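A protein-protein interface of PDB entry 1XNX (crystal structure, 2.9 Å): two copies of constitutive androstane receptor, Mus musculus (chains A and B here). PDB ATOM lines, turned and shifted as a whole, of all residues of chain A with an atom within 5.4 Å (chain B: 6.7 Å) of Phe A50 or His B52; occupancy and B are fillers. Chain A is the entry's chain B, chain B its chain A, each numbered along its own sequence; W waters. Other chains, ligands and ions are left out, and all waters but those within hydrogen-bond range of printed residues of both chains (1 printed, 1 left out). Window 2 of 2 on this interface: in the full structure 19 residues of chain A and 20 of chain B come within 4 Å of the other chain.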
ATOM      1  N   VAL A  41      17.496  -8.061  -0.071  1.00  0.00           N
ATOM      2  CA  VAL A  41      17.532  -9.527  -0.175  1.00  0.00           C
ATOM      3  C   VAL A  41      18.787 -10.016  -0.906  1.00  0.00           C
ATOM      4  O   VAL A  41      19.116 -11.200  -0.874  1.00  0.00           O
ATOM      5  CB  VAL A  41      16.304 -10.069  -0.946  1.00  0.00           C
ATOM      6  CG1 VAL A  41      16.440  -9.763  -2.432  1.00  0.00           C
ATOM      7  CG2 VAL A  41      16.162 -11.550  -0.706  1.00  0.00           C
ATOM      8  N   PRO A  45      21.329 -11.715   3.745  1.00  0.00           N
ATOM      9  CA  PRO A  45      20.595 -11.453   4.987  1.00  0.00           C
ATOM     10  C   PRO A  45      20.344 -12.763   5.728  1.00  0.00           C
ATOM     11  O   PRO A  45      19.892 -13.735   5.126  1.00  0.00           O
ATOM     12  CB  PRO A  45      19.295 -10.855   4.487  1.00  0.00           C
ATOM     13  CG  PRO A  45      19.056 -11.633   3.235  1.00  0.00           C
ATOM     14  CD  PRO A  45      20.427 -11.597   2.587  1.00  0.00           C
ATOM     15  N   PRO A  46      20.640 -12.810   7.040  1.00  0.00           N
ATOM     16  CA  PRO A  46      20.422 -14.035   7.817  1.00  0.00           C
ATOM     17  C   PRO A  46      18.997 -14.522   7.585  1.00  0.00           C
ATOM     18  O   PRO A  46      18.062 -13.717   7.521  1.00  0.00           O
ATOM     19  CB  PRO A  46      20.657 -13.578   9.252  1.00  0.00           C
ATOM     20  CG  PRO A  46      21.672 -12.481   9.090  1.00  0.00           C
ATOM     21  CD  PRO A  46      21.157 -11.726   7.896  1.00  0.00           C
ATOM     22  N   ALA A  47      18.830 -15.834   7.461  1.00  0.00           N
ATOM     23  CA  ALA A  47      17.517 -16.431   7.206  1.00  0.00           C
ATOM     24  C   ALA A  47      16.359 -15.887   8.043  1.00  0.00           C
ATOM     25  O   ALA A  47      15.264 -15.699   7.522  1.00  0.00           O
ATOM     26  CB  ALA A  47      17.598 -17.937   7.370  1.00  0.00           C
ATOM     27  N   TYR A  48      16.592 -15.616   9.323  1.00  0.00           N
ATOM     28  CA  TYR A  48      15.519 -15.121  10.181  1.00  0.00           C
ATOM     29  C   TYR A  48      14.900 -13.783   9.785  1.00  0.00           C
ATOM     30  O   TYR A  48      13.793 -13.466  10.215  1.00  0.00           O
ATOM     31  CB  TYR A  48      15.969 -15.071  11.654  1.00  0.00           C
ATOM     32  CG  TYR A  48      17.200 -14.233  11.937  1.00  0.00           C
ATOM     33  CD1 TYR A  48      17.146 -12.837  11.890  1.00  0.00           C
ATOM     34  CD2 TYR A  48      18.426 -14.839  12.251  1.00  0.00           C
ATOM     35  CE1 TYR A  48      18.279 -12.061  12.151  1.00  0.00           C
ATOM     36  CE2 TYR A  48      19.563 -14.074  12.511  1.00  0.00           C
ATOM     37  CZ  TYR A  48      19.481 -12.685  12.462  1.00  0.00           C
ATOM     38  OH  TYR A  48      20.588 -11.921  12.745  1.00  0.00           O
ATOM     39  N   LEU A  49      15.581 -12.989   8.969  1.00  0.00           N
ATOM     40  CA  LEU A  49      14.994 -11.710   8.571  1.00  0.00           C
ATOM     41  C   LEU A  49      13.863 -11.941   7.575  1.00  0.00           C
ATOM     42  O   LEU A  49      13.182 -10.992   7.176  1.00  0.00           O
ATOM     43  CB  LEU A  49      16.045 -10.789   7.942  1.00  0.00           C
ATOM     44  CG  LEU A  49      17.244 -10.356   8.794  1.00  0.00           C
ATOM     45  CD1 LEU A  49      18.245  -9.634   7.906  1.00  0.00           C
ATOM     46  CD2 LEU A  49      16.787  -9.464   9.949  1.00  0.00           C
ATOM     47  N   PHE A  50      13.666 -13.195   7.162  1.00  0.00           N
ATOM     48  CA  PHE A  50      12.600 -13.518   6.206  1.00  0.00           C
ATOM     49  C   PHE A  50      11.284 -13.766   6.913  1.00  0.00           C
ATOM     50  O   PHE A  50      10.236 -13.870   6.270  1.00  0.00           O
ATOM     51  CB  PHE A  50      12.926 -14.774   5.399  1.00  0.00           C
ATOM     52  CG  PHE A  50      13.913 -14.562   4.289  1.00  0.00           C
ATOM     53  CD1 PHE A  50      15.280 -14.713   4.512  1.00  0.00           C
ATOM     54  CD2 PHE A  50      13.473 -14.226   3.007  1.00  0.00           C
ATOM     55  CE1 PHE A  50      16.198 -14.537   3.464  1.00  0.00           C
ATOM     56  CE2 PHE A  50      14.377 -14.048   1.958  1.00  0.00           C
ATOM     57  CZ  PHE A  50      15.738 -14.203   2.189  1.00  0.00           C
ATOM     58  N   MET A  51      11.348 -13.859   8.240  1.00  0.00           N
ATOM     59  CA  MET A  51      10.181 -14.145   9.060  1.00  0.00           C
ATOM     60  C   MET A  51       9.660 -12.921   9.810  1.00  0.00           C
ATOM     61  O   MET A  51      10.448 -12.157  10.367  1.00  0.00           O
ATOM     62  CB  MET A  51      10.548 -15.245  10.046  1.00  0.00           C
ATOM     63  CG  MET A  51      11.245 -16.442   9.393  1.00  0.00           C
ATOM     64  SD  MET A  51      11.588 -17.806  10.560  1.00  0.00           S
ATOM     65  CE  MET A  51      12.970 -17.089  11.507  1.00  0.00           C
ATOM     66  N   HIS A  52       8.338 -12.745   9.841  1.00  0.00           N
ATOM     67  CA  HIS A  52       7.744 -11.599  10.520  1.00  0.00           C
ATOM     68  C   HIS A  52       7.434 -11.862  11.991  1.00  0.00           C
ATOM     69  O   HIS A  52       7.324 -10.931  12.790  1.00  0.00           O
ATOM     70  CB  HIS A  52       6.458 -11.143   9.801  1.00  0.00           C
ATOM     71  CG  HIS A  52       5.229 -11.917  10.186  1.00  0.00           C
ATOM     72  ND1 HIS A  52       4.944 -13.174   9.687  1.00  0.00           N
ATOM     73  CD2 HIS A  52       4.221 -11.615  11.040  1.00  0.00           C
ATOM     74  CE1 HIS A  52       3.816 -13.612  10.219  1.00  0.00           C
ATOM     75  NE2 HIS A  52       3.358 -12.685  11.044  1.00  0.00           N
ATOM     76  N   PHE A 126       9.119  -3.558   6.239  1.00  0.00           N
ATOM     77  CA  PHE A 126       9.000  -4.570   5.202  1.00  0.00           C
ATOM     78  C   PHE A 126       9.740  -4.160   3.933  1.00  0.00           C
ATOM     79  O   PHE A 126       9.258  -3.351   3.149  1.00  0.00           O
ATOM     80  CB  PHE A 126       7.519  -4.839   4.901  1.00  0.00           C
ATOM     81  CG  PHE A 126       6.754  -5.393   6.075  1.00  0.00           C
ATOM     82  CD1 PHE A 126       5.666  -4.704   6.606  1.00  0.00           C
ATOM     83  CD2 PHE A 126       7.134  -6.599   6.664  1.00  0.00           C
ATOM     84  CE1 PHE A 126       4.972  -5.206   7.704  1.00  0.00           C
ATOM     85  CE2 PHE A 126       6.444  -7.112   7.766  1.00  0.00           C
ATOM     86  CZ  PHE A 126       5.365  -6.417   8.287  1.00  0.00           C
ATOM     87  N   GLY A 128      11.104  -5.742   0.635  1.00  0.00           N
ATOM     88  CA  GLY A 128      11.113  -6.925  -0.201  1.00  0.00           C
ATOM     89  C   GLY A 128      10.564  -8.051   0.644  1.00  0.00           C
ATOM     90  O   GLY A 128       9.646  -7.818   1.414  1.00  0.00           O
ATOM     91  N   PRO A 129      11.095  -9.277   0.541  1.00  0.00           N
ATOM     92  CA  PRO A 129      10.582 -10.384   1.356  1.00  0.00           C
ATOM     93  C   PRO A 129      11.002 -10.280   2.836  1.00  0.00           C
ATOM     94  O   PRO A 129      10.509 -11.022   3.692  1.00  0.00           O
ATOM     95  CB  PRO A 129      11.184 -11.610   0.670  1.00  0.00           C
ATOM     96  CG  PRO A 129      12.521 -11.100   0.235  1.00  0.00           C
ATOM     97  CD  PRO A 129      12.184  -9.734  -0.341  1.00  0.00           C
ATOM     98  N   LEU A 130      11.902  -9.342   3.113  1.00  0.00           N
ATOM     99  CA  LEU A 130      12.456  -9.113   4.452  1.00  0.00           C
ATOM    100  C   LEU A 130      11.600  -8.348   5.475  1.00  0.00           C
ATOM    101  O   LEU A 130      10.789  -7.478   5.115  1.00  0.00           O
ATOM    102  CB  LEU A 130      13.813  -8.415   4.302  1.00  0.00           C
ATOM    103  CG  LEU A 130      15.033  -9.307   4.022  1.00  0.00           C
ATOM    104  CD1 LEU A 130      14.623 -10.601   3.333  1.00  0.00           C
ATOM    105  CD2 LEU A 130      16.053  -8.523   3.199  1.00  0.00           C
ATOM    106  N   CYS A 131      11.803  -8.682   6.751  1.00  0.00           N
ATOM    107  CA  CYS A 131      11.099  -8.044   7.864  1.00  0.00           C
ATOM    108  C   CYS A 131      12.091  -7.602   8.949  1.00  0.00           C
ATOM    109  O   CYS A 131      12.563  -8.427   9.732  1.00  0.00           O
ATOM    110  CB  CYS A 131      10.084  -9.014   8.481  1.00  0.00           C
ATOM    111  SG  CYS A 131       9.148  -8.353   9.907  1.00  0.00           S
ATOM    112  N   TYR B  48       0.695 -21.753   4.560  1.00  0.00           N
ATOM    113  CA  TYR B  48       1.008 -20.460   3.942  1.00  0.00           C
ATOM    114  C   TYR B  48       0.495 -19.266   4.749  1.00  0.00           C
ATOM    115  O   TYR B  48       0.956 -18.131   4.558  1.00  0.00           O
ATOM    116  CB  TYR B  48       0.484 -20.389   2.498  1.00  0.00           C
ATOM    117  CG  TYR B  48      -0.958 -20.816   2.312  1.00  0.00           C
ATOM    118  CD1 TYR B  48      -2.017 -19.917   2.509  1.00  0.00           C
ATOM    119  CD2 TYR B  48      -1.265 -22.127   1.956  1.00  0.00           C
ATOM    120  CE1 TYR B  48      -3.352 -20.326   2.352  1.00  0.00           C
ATOM    121  CE2 TYR B  48      -2.582 -22.544   1.802  1.00  0.00           C
ATOM    122  CZ  TYR B  48      -3.622 -21.648   1.998  1.00  0.00           C
ATOM    123  OH  TYR B  48      -4.919 -22.092   1.831  1.00  0.00           O
ATOM    124  N   LEU B  49      -0.448 -19.512   5.652  1.00  0.00           N
ATOM    125  CA  LEU B  49      -0.967 -18.437   6.477  1.00  0.00           C
ATOM    126  C   LEU B  49       0.139 -17.892   7.375  1.00  0.00           C
ATOM    127  O   LEU B  49       0.055 -16.754   7.854  1.00  0.00           O
ATOM    128  CB  LEU B  49      -2.130 -18.938   7.333  1.00  0.00           C
ATOM    129  CG  LEU B  49      -3.576 -18.611   6.921  1.00  0.00           C
ATOM    130  CD1 LEU B  49      -3.728 -18.442   5.415  1.00  0.00           C
ATOM    131  CD2 LEU B  49      -4.469 -19.723   7.432  1.00  0.00           C
ATOM    132  N   PHE B  50       1.173 -18.702   7.606  1.00  0.00           N
ATOM    133  CA  PHE B  50       2.295 -18.287   8.451  1.00  0.00           C
ATOM    134  C   PHE B  50       3.294 -17.381   7.740  1.00  0.00           C
ATOM    135  O   PHE B  50       4.175 -16.812   8.390  1.00  0.00           O
ATOM    136  CB  PHE B  50       3.067 -19.490   8.981  1.00  0.00           C
ATOM    137  CG  PHE B  50       2.353 -20.267  10.044  1.00  0.00           C
ATOM    138  CD1 PHE B  50       1.445 -21.271   9.709  1.00  0.00           C
ATOM    139  CD2 PHE B  50       2.622 -20.030  11.392  1.00  0.00           C
ATOM    140  CE1 PHE B  50       0.822 -22.032  10.711  1.00  0.00           C
ATOM    141  CE2 PHE B  50       2.006 -20.780  12.388  1.00  0.00           C
ATOM    142  CZ  PHE B  50       1.105 -21.781  12.045  1.00  0.00           C
ATOM    143  N   MET B  51       3.176 -17.253   6.419  1.00  0.00           N
ATOM    144  CA  MET B  51       4.101 -16.424   5.655  1.00  0.00           C
ATOM    145  C   MET B  51       3.518 -15.049   5.373  1.00  0.00           C
ATOM    146  O   MET B  51       2.364 -14.936   4.959  1.00  0.00           O
ATOM    147  CB  MET B  51       4.436 -17.094   4.329  1.00  0.00           C
ATOM    148  CG  MET B  51       5.098 -18.463   4.446  1.00  0.00           C
ATOM    149  SD  MET B  51       5.362 -19.207   2.806  1.00  0.00           S
ATOM    150  CE  MET B  51       6.909 -18.462   2.349  1.00  0.00           C
ATOM    151  N   HIS B  52       4.304 -13.996   5.576  1.00  0.00           N
ATOM    152  CA  HIS B  52       3.774 -12.663   5.322  1.00  0.00           C
ATOM    153  C   HIS B  52       4.045 -12.257   3.890  1.00  0.00           C
ATOM    154  O   HIS B  52       3.298 -11.473   3.311  1.00  0.00           O
ATOM    155  CB  HIS B  52       4.381 -11.623   6.274  1.00  0.00           C
ATOM    156  CG  HIS B  52       5.789 -11.238   5.937  1.00  0.00           C
ATOM    157  ND1 HIS B  52       6.855 -12.105   6.075  1.00  0.00           N
ATOM    158  CD2 HIS B  52       6.306 -10.077   5.471  1.00  0.00           C
ATOM    159  CE1 HIS B  52       7.967 -11.491   5.712  1.00  0.00           C
ATOM    160  NE2 HIS B  52       7.662 -10.261   5.341  1.00  0.00           N
ATOM    161  N   HIS B  53       5.121 -12.789   3.324  1.00  0.00           N
ATOM    162  CA  HIS B  53       5.487 -12.476   1.950  1.00  0.00           C
ATOM    163  C   HIS B  53       5.366 -13.736   1.097  1.00  0.00           C
ATOM    164  O   HIS B  53       6.180 -14.655   1.225  1.00  0.00           O
ATOM    165  CB  HIS B  53       6.919 -11.957   1.892  1.00  0.00           C
ATOM    166  CG  HIS B  53       7.314 -11.445   0.545  1.00  0.00           C
ATOM    167  ND1 HIS B  53       6.964 -10.190   0.094  1.00  0.00           N
ATOM    168  CD2 HIS B  53       7.994 -12.036  -0.467  1.00  0.00           C
ATOM    169  CE1 HIS B  53       7.412 -10.027  -1.138  1.00  0.00           C
ATOM    170  NE2 HIS B  53       8.040 -11.132  -1.502  1.00  0.00           N
ATOM    171  N   ARG B  54       4.364 -13.782   0.224  1.00  0.00           N
ATOM    172  CA  ARG B  54       4.159 -14.970  -0.607  1.00  0.00           C
ATOM    173  C   ARG B  54       3.482 -14.664  -1.934  1.00  0.00           C
ATOM    174  O   ARG B  54       2.466 -15.269  -2.273  1.00  0.00           O
ATOM    175  CB  ARG B  54       3.318 -15.992   0.164  1.00  0.00           C
ATOM    176  CG  ARG B  54       2.433 -15.365   1.216  1.00  0.00           C
ATOM    177  CD  ARG B  54       1.274 -16.259   1.596  1.00  0.00           C
ATOM    178  NE  ARG B  54       0.535 -15.718   2.728  1.00  0.00           N
ATOM    179  CZ  ARG B  54      -0.786 -15.766   2.853  1.00  0.00           C
ATOM    180  NH1 ARG B  54      -1.519 -16.333   1.905  1.00  0.00           N
ATOM    181  NH2 ARG B  54      -1.372 -15.250   3.930  1.00  0.00           N
ATOM    182  N   PRO B  55       4.056 -13.744  -2.722  1.00  0.00           N
ATOM    183  CA  PRO B  55       3.490 -13.357  -4.018  1.00  0.00           C
ATOM    184  C   PRO B  55       3.135 -14.480  -4.998  1.00  0.00           C
ATOM    185  O   PRO B  55       2.116 -14.399  -5.688  1.00  0.00           O
ATOM    186  CB  PRO B  55       4.551 -12.417  -4.589  1.00  0.00           C
ATOM    187  CG  PRO B  55       5.809 -12.962  -4.022  1.00  0.00           C
ATOM    188  CD  PRO B  55       5.430 -13.230  -2.583  1.00  0.00           C
ATOM    189  N   ASN B 124      -2.982  -6.154   5.459  1.00  0.00           N
ATOM    190  CA  ASN B 124      -2.992  -7.526   5.937  1.00  0.00           C
ATOM    191  C   ASN B 124      -3.252  -7.493   7.428  1.00  0.00           C
ATOM    192  O   ASN B 124      -2.883  -6.525   8.095  1.00  0.00           O
ATOM    193  CB  ASN B 124      -1.651  -8.201   5.677  1.00  0.00           C
ATOM    194  CG  ASN B 124      -1.398  -8.432   4.209  1.00  0.00           C
ATOM    195  OD1 ASN B 124      -2.326  -8.674   3.442  1.00  0.00           O
ATOM    196  ND2 ASN B 124      -0.136  -8.378   3.811  1.00  0.00           N
ATOM    197  N   PHE B 126      -2.471  -9.019  11.065  1.00  0.00           N
ATOM    198  CA  PHE B 126      -1.447  -9.810  11.745  1.00  0.00           C
ATOM    199  C   PHE B 126      -2.008 -10.353  13.047  1.00  0.00           C
ATOM    200  O   PHE B 126      -2.081  -9.633  14.057  1.00  0.00           O
ATOM    201  CB  PHE B 126      -0.202  -8.976  12.027  1.00  0.00           C
ATOM    202  CG  PHE B 126       0.576  -8.627  10.793  1.00  0.00           C
ATOM    203  CD1 PHE B 126       0.139  -7.625   9.941  1.00  0.00           C
ATOM    204  CD2 PHE B 126       1.718  -9.346  10.449  1.00  0.00           C
ATOM    205  CE1 PHE B 126       0.833  -7.344   8.755  1.00  0.00           C
ATOM    206  CE2 PHE B 126       2.409  -9.073   9.275  1.00  0.00           C
ATOM    207  CZ  PHE B 126       1.968  -8.071   8.423  1.00  0.00           C
ATOM    208  N   CYS B 131      -0.705 -14.342   9.028  1.00  0.00           N
ATOM    209  CA  CYS B 131      -0.836 -13.136   8.223  1.00  0.00           C
ATOM    210  C   CYS B 131      -1.944 -13.315   7.179  1.00  0.00           C
ATOM    211  O   CYS B 131      -1.769 -14.020   6.186  1.00  0.00           O
ATOM    212  CB  CYS B 131       0.490 -12.808   7.533  1.00  0.00           C
ATOM    213  SG  CYS B 131       0.379 -11.370   6.453  1.00  0.00           S
ATOM    214  N   LYS B 133      -4.448 -12.270   4.140  1.00  0.00           N
ATOM    215  CA  LYS B 133      -4.474 -11.443   2.949  1.00  0.00           C
ATOM    216  C   LYS B 133      -5.851 -11.603   2.329  1.00  0.00           C
ATOM    217  O   LYS B 133      -6.464 -12.673   2.437  1.00  0.00           O
ATOM    218  CB  LYS B 133      -3.410 -11.914   1.963  1.00  0.00           C
ATOM    219  CG  LYS B 133      -2.010 -11.943   2.544  1.00  0.00           C
ATOM    220  CD  LYS B 133      -1.043 -12.599   1.586  1.00  0.00           C
ATOM    221  CE  LYS B 133       0.368 -12.456   2.077  1.00  0.00           C
ATOM    222  NZ  LYS B 133       0.657 -11.027   2.365  1.00  0.00           N
HETATM  223  O   HOH W   1       6.721 -14.097   7.653  1.00  0.00           O
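Of chain B, only His B52 (3.3 Å) comes within 4 Å of Phe A50.
Of chain A, only Phe A50 (3.3 Å), His A52 (3.8 Å), Phe A126 (3.8 Å) and Pro A129 (3.3 Å) come within 4 Å of His B52.
Printed residues of chain B within 4 Å of His A52: Phe B50 (3.7 Å), His B52 (3.8 Å) and Phe B126 (3.4 Å).
Printed residues of chain A within 4 Å of Phe B50: His A52.
Leu A49 touches none of the printed residues of chain B.
The nearest residue of chain A that does not touch His B52 is Cys A131 (4.2 Å).
Phe A50 touches His B52, and with the chains exchanged His A52 touches Phe B50.
His A52 touches its own counterpart, His B52.
His A52 touches Phe B126, and with the chains exchanged Phe A126 touches His B52.
Phe B126 touches its own counterpart, Phe A126.
7 positions are printed for both chains.
Of the 9 pairs that touch across the chains among the printed residues, 6 have their exchanged pair printed and touching as well.
NZ of Lys B133 lies within hydrogen-bond range of O of His B52 (2.8 Å).
NE2 of His B52 sits close to O of Pro A129, at 3.4 Å.
Hydrophobic or aromatic side chains of chain B within 4 Å of the printed part of chain A: His B52, His B53 and Phe B126.
Hydrophobic or aromatic side chains of chain A that line the printed part of chain B: His A52, Phe A126 and Pro A129.
Among the printed residues, no Asp or Glu carboxylate lies within 4 Å of a Lys or Arg side-chain nitrogen of the other chain.
Water W1 lies within hydrogen-bond range of a ring nitrogen (ND1) of His B52 and a ring nitrogen (ND1) of His A52.
O of Phe A50 touches CE1 of His B52, 3.3 Å away.
O of Phe B50 touches CE1 of His A52 (3.7 Å).
His A52 touches His B52.
CD2 of His A52 touches CD2 of Phe B126, at 3.4 Å.
CE2 of Phe A126 touches CD2 of His B52 (3.8 Å).
Phe A126 touches Phe B126.
His B53 touches Gly A128.
Pro A129 touches His B53.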
